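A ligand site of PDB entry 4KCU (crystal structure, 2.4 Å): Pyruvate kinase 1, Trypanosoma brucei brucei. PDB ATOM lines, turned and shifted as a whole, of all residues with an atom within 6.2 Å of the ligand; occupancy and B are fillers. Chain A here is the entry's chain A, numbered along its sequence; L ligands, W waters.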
ATOM      1  N   VAL A 399      17.347  20.361  -7.538  1.00  0.00           N
ATOM      2  CA  VAL A 399      16.615  19.236  -7.004  1.00  0.00           C
ATOM      3  C   VAL A 399      16.168  19.525  -5.568  1.00  0.00           C
ATOM      4  O   VAL A 399      16.902  20.150  -4.815  1.00  0.00           O
ATOM      5  CB  VAL A 399      17.443  17.975  -7.042  1.00  0.00           C
ATOM      6  CG1 VAL A 399      18.729  18.157  -6.225  1.00  0.00           C
ATOM      7  CG2 VAL A 399      16.635  16.792  -6.559  1.00  0.00           C
ATOM      8  N   LEU A 400      14.935  19.139  -5.228  1.00  0.00           N
ATOM      9  CA  LEU A 400      14.492  19.149  -3.848  1.00  0.00           C
ATOM     10  C   LEU A 400      14.898  17.877  -3.154  1.00  0.00           C
ATOM     11  O   LEU A 400      14.517  16.767  -3.558  1.00  0.00           O
ATOM     12  CB  LEU A 400      12.976  19.330  -3.741  1.00  0.00           C
ATOM     13  CG  LEU A 400      12.469  20.770  -3.882  1.00  0.00           C
ATOM     14  CD1 LEU A 400      13.238  21.537  -4.955  1.00  0.00           C
ATOM     15  CD2 LEU A 400      10.970  20.783  -4.160  1.00  0.00           C
ATOM     16  N   SER A 401      15.650  18.028  -2.082  1.00  0.00           N
ATOM     17  CA  SER A 401      16.033  16.848  -1.318  1.00  0.00           C
ATOM     18  C   SER A 401      16.027  17.149   0.159  1.00  0.00           C
ATOM     19  O   SER A 401      16.672  18.107   0.602  1.00  0.00           O
ATOM     20  CB  SER A 401      17.415  16.315  -1.764  1.00  0.00           C
ATOM     21  OG  SER A 401      17.639  14.999  -1.271  1.00  0.00           O
ATOM     22  N   ASN A 402      15.335  16.324   0.931  1.00  0.00           N
ATOM     23  CA  ASN A 402      15.320  16.465   2.374  1.00  0.00           C
ATOM     24  C   ASN A 402      16.382  15.635   3.074  1.00  0.00           C
ATOM     25  O   ASN A 402      17.117  16.136   3.951  1.00  0.00           O
ATOM     26  CB  ASN A 402      13.911  16.193   2.925  1.00  0.00           C
ATOM     27  CG  ASN A 402      12.867  17.048   2.248  1.00  0.00           C
ATOM     28  OD1 ASN A 402      13.088  18.230   2.063  1.00  0.00           O
ATOM     29  ND2 ASN A 402      11.840  16.422   1.705  1.00  0.00           N
ATOM     30  N   THR A 403      16.501  14.357   2.668  1.00  0.00           N
ATOM     31  CA  THR A 403      17.531  13.489   3.271  1.00  0.00           C
ATOM     32  C   THR A 403      18.862  13.622   2.557  1.00  0.00           C
ATOM     33  O   THR A 403      19.908  13.184   3.085  1.00  0.00           O
ATOM     34  CB  THR A 403      17.149  12.030   3.216  1.00  0.00           C
ATOM     35  OG1 THR A 403      17.055  11.628   1.829  1.00  0.00           O
ATOM     36  CG2 THR A 403      15.769  11.775   3.956  1.00  0.00           C
ATOM     37  N   GLY A 404      18.843  14.166   1.326  1.00  0.00           N
ATOM     38  CA  GLY A 404      20.030  14.172   0.479  1.00  0.00           C
ATOM     39  C   GLY A 404      20.044  13.060  -0.543  1.00  0.00           C
ATOM     40  O   GLY A 404      20.740  13.158  -1.543  1.00  0.00           O
ATOM     41  N   ARG A 405      19.201  12.040  -0.365  1.00  0.00           N
ATOM     42  CA  ARG A 405      19.185  10.908  -1.285  1.00  0.00           C
ATOM     43  C   ARG A 405      19.079  11.323  -2.771  1.00  0.00           C
ATOM     44  O   ARG A 405      19.853  10.827  -3.620  1.00  0.00           O
ATOM     45  CB  ARG A 405      18.080   9.912  -0.941  1.00  0.00           C
ATOM     46  CG  ARG A 405      18.183   8.633  -1.753  1.00  0.00           C
ATOM     47  CD  ARG A 405      16.841   7.929  -1.958  1.00  0.00           C
ATOM     48  NE  ARG A 405      16.959   6.900  -3.007  1.00  0.00           N
ATOM     49  CZ  ARG A 405      16.032   6.007  -3.303  1.00  0.00           C
ATOM     50  NH1 ARG A 405      16.247   5.112  -4.261  1.00  0.00           N
ATOM     51  NH2 ARG A 405      14.868   6.019  -2.668  1.00  0.00           N
ATOM     52  N   SER A 406      18.129  12.206  -3.087  1.00  0.00           N
ATOM     53  CA  SER A 406      17.911  12.583  -4.485  1.00  0.00           C
ATOM     54  C   SER A 406      19.086  13.383  -5.031  1.00  0.00           C
ATOM     55  O   SER A 406      19.452  13.226  -6.203  1.00  0.00           O
ATOM     56  CB  SER A 406      16.613  13.384  -4.651  1.00  0.00           C
ATOM     57  OG  SER A 406      15.484  12.643  -4.168  1.00  0.00           O
ATOM     58  N   ALA A 407      19.688  14.227  -4.202  1.00  0.00           N
ATOM     59  CA  ALA A 407      20.864  14.975  -4.628  1.00  0.00           C
ATOM     60  C   ALA A 407      22.031  14.012  -4.917  1.00  0.00           C
ATOM     61  O   ALA A 407      22.726  14.153  -5.909  1.00  0.00           O
ATOM     62  CB  ALA A 407      21.257  16.019  -3.581  1.00  0.00           C
ATOM     63  N   THR A 424      15.430  20.900   3.382  1.00  0.00           N
ATOM     64  CA  THR A 424      14.729  21.379   4.542  1.00  0.00           C
ATOM     65  C   THR A 424      15.492  21.046   5.847  1.00  0.00           C
ATOM     66  O   THR A 424      14.994  21.285   6.956  1.00  0.00           O
ATOM     67  CB  THR A 424      13.301  20.792   4.595  1.00  0.00           C
ATOM     68  OG1 THR A 424      13.384  19.363   4.491  1.00  0.00           O
ATOM     69  CG2 THR A 424      12.466  21.317   3.434  1.00  0.00           C
ATOM     70  N   GLU A 450       4.824  24.865   4.537  1.00  0.00           N
ATOM     71  CA  GLU A 450       4.975  23.500   4.124  1.00  0.00           C
ATOM     72  C   GLU A 450       5.452  23.322   2.659  1.00  0.00           C
ATOM     73  O   GLU A 450       6.197  22.371   2.351  1.00  0.00           O
ATOM     74  CB  GLU A 450       3.680  22.728   4.377  1.00  0.00           C
ATOM     75  CG  GLU A 450       3.569  22.237   5.799  1.00  0.00           C
ATOM     76  CD  GLU A 450       2.165  21.745   6.167  1.00  0.00           C
ATOM     77  OE1 GLU A 450       1.266  21.736   5.286  1.00  0.00           O
ATOM     78  OE2 GLU A 450       1.974  21.388   7.354  1.00  0.00           O
ATOM     79  N   ASP A 451       5.002  24.189   1.770  1.00  0.00           N
ATOM     80  CA  ASP A 451       5.448  24.131   0.359  1.00  0.00           C
ATOM     81  C   ASP A 451       5.066  22.828  -0.349  1.00  0.00           C
ATOM     82  O   ASP A 451       5.874  22.237  -1.059  1.00  0.00           O
ATOM     83  CB  ASP A 451       6.963  24.385   0.249  1.00  0.00           C
ATOM     84  CG  ASP A 451       7.380  24.873  -1.158  1.00  0.00           C
ATOM     85  OD1 ASP A 451       6.623  25.638  -1.775  1.00  0.00           O
ATOM     86  OD2 ASP A 451       8.496  24.484  -1.638  1.00  0.00           O
ATOM     87  N   LYS A 452       3.817  22.413  -0.177  1.00  0.00           N
ATOM     88  CA  LYS A 452       3.343  21.164  -0.802  1.00  0.00           C
ATOM     89  C   LYS A 452       3.464  21.191  -2.328  1.00  0.00           C
ATOM     90  O   LYS A 452       3.764  20.186  -2.945  1.00  0.00           O
ATOM     91  CB  LYS A 452       1.907  20.865  -0.382  1.00  0.00           C
ATOM     92  CG  LYS A 452       1.756  20.407   1.058  1.00  0.00           C
ATOM     93  CD  LYS A 452       0.290  20.357   1.465  1.00  0.00           C
ATOM     94  CE  LYS A 452       0.110  19.878   2.902  1.00  0.00           C
ATOM     95  NZ  LYS A 452       1.055  18.788   3.258  1.00  0.00           N
ATOM     96  N   LYS A 454       5.708  22.935  -3.943  1.00  0.00           N
ATOM     97  CA  LYS A 454       7.152  23.078  -4.281  1.00  0.00           C
ATOM     98  C   LYS A 454       7.556  24.447  -4.813  1.00  0.00           C
ATOM     99  O   LYS A 454       8.728  24.720  -4.963  1.00  0.00           O
ATOM    100  CB  LYS A 454       7.646  21.979  -5.250  1.00  0.00           C
ATOM    101  CG  LYS A 454       6.775  20.737  -5.337  1.00  0.00           C
ATOM    102  CD  LYS A 454       6.927  19.854  -4.123  1.00  0.00           C
ATOM    103  CE  LYS A 454       6.245  18.503  -4.342  1.00  0.00           C
ATOM    104  NZ  LYS A 454       5.771  17.929  -3.053  1.00  0.00           N
ATOM    105  N   ARG A 457      10.268  26.432  -2.775  1.00  0.00           N
ATOM    106  CA  ARG A 457      11.622  25.925  -2.810  1.00  0.00           C
ATOM    107  C   ARG A 457      12.276  26.073  -4.187  1.00  0.00           C
ATOM    108  O   ARG A 457      13.460  26.359  -4.280  1.00  0.00           O
ATOM    109  CB  ARG A 457      11.664  24.502  -2.327  1.00  0.00           C
ATOM    110  CG  ARG A 457      11.346  24.389  -0.856  1.00  0.00           C
ATOM    111  CD  ARG A 457      11.275  22.958  -0.418  1.00  0.00           C
ATOM    112  NE  ARG A 457       9.992  22.376  -0.748  1.00  0.00           N
ATOM    113  CZ  ARG A 457       9.713  21.088  -0.589  1.00  0.00           C
ATOM    114  NH1 ARG A 457      10.650  20.247  -0.183  1.00  0.00           N
ATOM    115  NH2 ARG A 457       8.474  20.634  -0.815  1.00  0.00           N
ATOM    116  N   VAL A 480      14.065  18.917 -10.571  1.00  0.00           N
ATOM    117  CA  VAL A 480      13.657  17.574 -10.247  1.00  0.00           C
ATOM    118  C   VAL A 480      13.000  17.584  -8.858  1.00  0.00           C
ATOM    119  O   VAL A 480      13.629  17.998  -7.908  1.00  0.00           O
ATOM    120  CB  VAL A 480      14.899  16.623 -10.219  1.00  0.00           C
ATOM    121  CG1 VAL A 480      14.545  15.247  -9.629  1.00  0.00           C
ATOM    122  CG2 VAL A 480      15.433  16.441 -11.639  1.00  0.00           C
ATOM    123  N   HIS A 481      11.729  17.205  -8.764  1.00  0.00           N
ATOM    124  CA  HIS A 481      11.103  16.950  -7.440  1.00  0.00           C
ATOM    125  C   HIS A 481       9.896  16.082  -7.661  1.00  0.00           C
ATOM    126  O   HIS A 481       9.770  15.464  -8.732  1.00  0.00           O
ATOM    127  CB  HIS A 481      10.705  18.271  -6.761  1.00  0.00           C
ATOM    128  CG  HIS A 481       9.942  19.211  -7.655  1.00  0.00           C
ATOM    129  ND1 HIS A 481       8.638  19.023  -7.964  1.00  0.00           N
ATOM    130  CD2 HIS A 481      10.311  20.449  -8.205  1.00  0.00           C
ATOM    131  CE1 HIS A 481       8.212  20.041  -8.740  1.00  0.00           C
ATOM    132  NE2 HIS A 481       9.235  20.926  -8.880  1.00  0.00           N
ATOM    133  N   ALA A 482       8.986  15.980  -6.694  1.00  0.00           N
ATOM    134  CA  ALA A 482       7.734  15.227  -6.958  1.00  0.00           C
ATOM    135  C   ALA A 482       6.657  16.113  -7.567  1.00  0.00           C
ATOM    136  O   ALA A 482       6.714  17.320  -7.469  1.00  0.00           O
ATOM    137  CB  ALA A 482       7.217  14.521  -5.692  1.00  0.00           C
ATOM    138  N   ASP A 483       5.680  15.506  -8.226  1.00  0.00           N
ATOM    139  CA  ASP A 483       4.465  16.200  -8.585  1.00  0.00           C
ATOM    140  C   ASP A 483       3.606  16.464  -7.338  1.00  0.00           C
ATOM    141  O   ASP A 483       4.010  16.174  -6.198  1.00  0.00           O
ATOM    142  CB  ASP A 483       3.678  15.407  -9.640  1.00  0.00           C
ATOM    143  CG  ASP A 483       3.121  14.067  -9.094  1.00  0.00           C
ATOM    144  OD1 ASP A 483       2.777  13.957  -7.887  1.00  0.00           O
ATOM    145  OD2 ASP A 483       2.970  13.138  -9.927  1.00  0.00           O
ATOM    146  N   VAL A 486       2.800  12.641  -5.175  1.00  0.00           N
ATOM    147  CA  VAL A 486       3.783  11.650  -4.757  1.00  0.00           C
ATOM    148  C   VAL A 486       4.630  12.106  -3.546  1.00  0.00           C
ATOM    149  O   VAL A 486       5.072  13.265  -3.473  1.00  0.00           O
ATOM    150  CB  VAL A 486       4.650  11.210  -5.935  1.00  0.00           C
ATOM    151  CG1 VAL A 486       5.777  10.287  -5.485  1.00  0.00           C
ATOM    152  CG2 VAL A 486       3.780  10.514  -7.000  1.00  0.00           C
ATOM    153  N   LYS A 487       4.714  11.256  -2.532  1.00  0.00           N
ATOM    154  CA  LYS A 487       5.541  11.534  -1.348  1.00  0.00           C
ATOM    155  C   LYS A 487       6.619  10.480  -1.199  1.00  0.00           C
ATOM    156  O   LYS A 487       6.334   9.278  -1.286  1.00  0.00           O
ATOM    157  CB  LYS A 487       4.691  11.543  -0.070  1.00  0.00           C
ATOM    158  CG  LYS A 487       3.429  12.406  -0.156  1.00  0.00           C
ATOM    159  CD  LYS A 487       3.650  13.863   0.267  1.00  0.00           C
ATOM    160  CE  LYS A 487       2.508  14.731  -0.282  1.00  0.00           C
ATOM    161  NZ  LYS A 487       2.904  16.150  -0.590  1.00  0.00           N
ATOM    162  N   GLY A 488       7.854  10.923  -0.920  1.00  0.00           N
ATOM    163  CA  GLY A 488       8.906   9.987  -0.560  1.00  0.00           C
ATOM    164  C   GLY A 488      10.071   9.974  -1.527  1.00  0.00           C
ATOM    165  O   GLY A 488      11.182   9.576  -1.168  1.00  0.00           O
ATOM    166  N   TYR A 489       9.851  10.485  -2.740  1.00  0.00           N
ATOM    167  CA  TYR A 489      10.932  10.518  -3.719  1.00  0.00           C
ATOM    168  C   TYR A 489      10.525  11.431  -4.844  1.00  0.00           C
ATOM    169  O   TYR A 489       9.377  11.803  -4.920  1.00  0.00           O
ATOM    170  CB  TYR A 489      11.171   9.101  -4.249  1.00  0.00           C
ATOM    171  CG  TYR A 489       9.938   8.499  -4.889  1.00  0.00           C
ATOM    172  CD1 TYR A 489       8.933   7.913  -4.100  1.00  0.00           C
ATOM    173  CD2 TYR A 489       9.698   8.644  -6.269  1.00  0.00           C
ATOM    174  CE1 TYR A 489       7.784   7.393  -4.689  1.00  0.00           C
ATOM    175  CE2 TYR A 489       8.558   8.134  -6.858  1.00  0.00           C
ATOM    176  CZ  TYR A 489       7.611   7.475  -6.085  1.00  0.00           C
ATOM    177  OH  TYR A 489       6.463   6.993  -6.690  1.00  0.00           O
ATOM    178  N   PRO A 490      11.440  11.727  -5.765  1.00  0.00           N
ATOM    179  CA  PRO A 490      10.993  12.614  -6.851  1.00  0.00           C
ATOM    180  C   PRO A 490      10.485  11.792  -8.039  1.00  0.00           C
ATOM    181  O   PRO A 490      11.143  10.871  -8.451  1.00  0.00           O
ATOM    182  CB  PRO A 490      12.276  13.356  -7.236  1.00  0.00           C
ATOM    183  CG  PRO A 490      13.355  12.391  -6.893  1.00  0.00           C
ATOM    184  CD  PRO A 490      12.906  11.617  -5.683  1.00  0.00           C
ATOM    185  N   ASN A 491       9.292  12.086  -8.566  1.00  0.00           N
ATOM    186  CA  ASN A 491       8.815  11.344  -9.755  1.00  0.00           C
ATOM    187  C   ASN A 491       8.752  12.199 -11.016  1.00  0.00           C
ATOM    188  O   ASN A 491       8.269  11.745 -12.067  1.00  0.00           O
ATOM    189  CB  ASN A 491       7.458  10.701  -9.479  1.00  0.00           C
ATOM    190  CG  ASN A 491       6.365  11.722  -9.383  1.00  0.00           C
ATOM    191  OD1 ASN A 491       6.549  12.773  -8.753  1.00  0.00           O
ATOM    192  ND2 ASN A 491       5.259  11.496 -10.089  1.00  0.00           N
HETATM  193  P1  LIG L   1       8.762  16.961  -0.647  1.00  0.00           P
HETATM  194  O1  LIG L   1       8.209  17.781  -1.769  1.00  0.00           O
HETATM  195  O2  LIG L   1       9.577  17.788   0.429  1.00  0.00           O
HETATM  196  O3  LIG L   1       7.634  16.161   0.085  1.00  0.00           O
HETATM  197  O4  LIG L   1       7.989  13.637  -0.927  1.00  0.00           O
HETATM  198  C1  LIG L   1       8.131  14.413  -2.151  1.00  0.00           C
HETATM  199  C2  LIG L   1       9.580  14.931  -2.175  1.00  0.00           C
HETATM  200  O5  LIG L   1       9.837  15.880  -1.144  1.00  0.00           O
HETATM  201  C3  LIG L   1      10.026  15.445  -3.538  1.00  0.00           C
HETATM  202  O6  LIG L   1       9.498  16.716  -3.851  1.00  0.00           O
HETATM  203  C4  LIG L   1      11.485  15.589  -3.244  1.00  0.00           C
HETATM  204  O7  LIG L   1      12.212  15.746  -4.484  1.00  0.00           O
HETATM  205  C5  LIG L   1      11.763  14.211  -2.596  1.00  0.00           C
HETATM  206  O8  LIG L   1      10.491  13.868  -1.913  1.00  0.00           O
HETATM  207  C6  LIG L   1      12.898  14.284  -1.660  1.00  0.00           C
HETATM  208  O9  LIG L   1      13.283  12.980  -1.226  1.00  0.00           O
HETATM  209  P2  LIG L   1      14.715  12.775  -0.556  1.00  0.00           P
HETATM  210  O10 LIG L   1      15.858  13.131  -1.467  1.00  0.00           O
HETATM  211  O11 LIG L   1      14.706  13.737   0.676  1.00  0.00           O
HETATM  212  O12 LIG L   1      14.787  11.241  -0.046  1.00  0.00           O
HETATM  213  O   HOH W   1      12.557  10.371   1.363  1.00  0.00           O
HETATM  214  O   HOH W   2      13.910   9.531  -1.778  1.00  0.00           O
HETATM  215  O   HOH W   3       8.563  18.886   2.775  1.00  0.00           O
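The side-chain hydroxyl (OG) of Ser 401 sits at hydrogen-bond distance from an oxygen (O10) of the ligand (2.6 Å). An oxygen (O11) of the ligand sits at hydrogen-bond distance from the backbone NH (N) of Asn 402 (2.7 Å). The side-chain amide nitrogen of Asn 402 lies within hydrogen-bond range of an oxygen (O2) of the ligand (2.9 Å). O of Leu 400 is in hydrogen-bond range of O7 of the ligand, at 2.7 Å. An oxygen (O4) of the ligand lies within hydrogen-bond range of the backbone NH (N) of Gly 488. NH1 of Arg 457 lies within salt-bridge range of O2 of the ligand. The backbone NH (N) of Thr 403 sits at hydrogen-bond distance from an oxygen (O11) of the ligand (2.8 Å). OG1 of Thr 403 is in hydrogen-bond range of O12 of the ligand (3.0 Å). An oxygen (O1) of the ligand is in salt-bridge range of the side-chain amino group (NZ) of Lys 454 (2.8 Å). The backbone NH (N) of Ser 406 sits at hydrogen-bond distance from an oxygen (O10) of the ligand, at 2.9 Å. An oxygen (O10) of the ligand is in hydrogen-bond range of the side-chain hydroxyl (OG) of Ser 406 (2.8 Å). O6 of the ligand is in hydrogen-bond range of N of Ala 482 (3.0 Å).
Merely in contact with the ligand: Arg 405, His 481, Val 486, Lys 487, Tyr 489 and Pro 490. Hydrophobic or aromatic side chains that line the ligand: Leu 400, His 481, Ala 482 and Pro 490.
Water W2 bridges an oxygen (O12) of the ligand (2.6 Å) and the backbone carbonyl oxygen (O) of Gly 488 (2.8 Å). Water W1 lies within hydrogen-bond range of O12 of the ligand (2.8 Å) and O of Gly 488 (3.0 Å).
OG of Ser 401 lies within hydrogen-bond range of N of Ser 406 (3.4 Å). The side-chain hydroxyl (OG) of Ser 401 is in hydrogen-bond range of the backbone NH (N) of Arg 405. N of Gly 404 lies within hydrogen-bond range of OG of Ser 401 (3.0 Å). OD1 of Asn 402 is in hydrogen-bond range of OG1 of Thr 424 (2.7 Å). The backbone carbonyl oxygen (O) of Val 480 lies within hydrogen-bond range of the backbone NH (N) of Leu 400. The side-chain carboxylate of Asp 451 is in salt-bridge range of the guanidinium group of Arg 457. The backbone NH (N) of Arg 405 lies within hydrogen-bond range of the side-chain hydroxyl (OG1) of Thr 403. NZ of Lys 454 is in hydrogen-bond range of O of Lys 452, at 3.0 Å.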
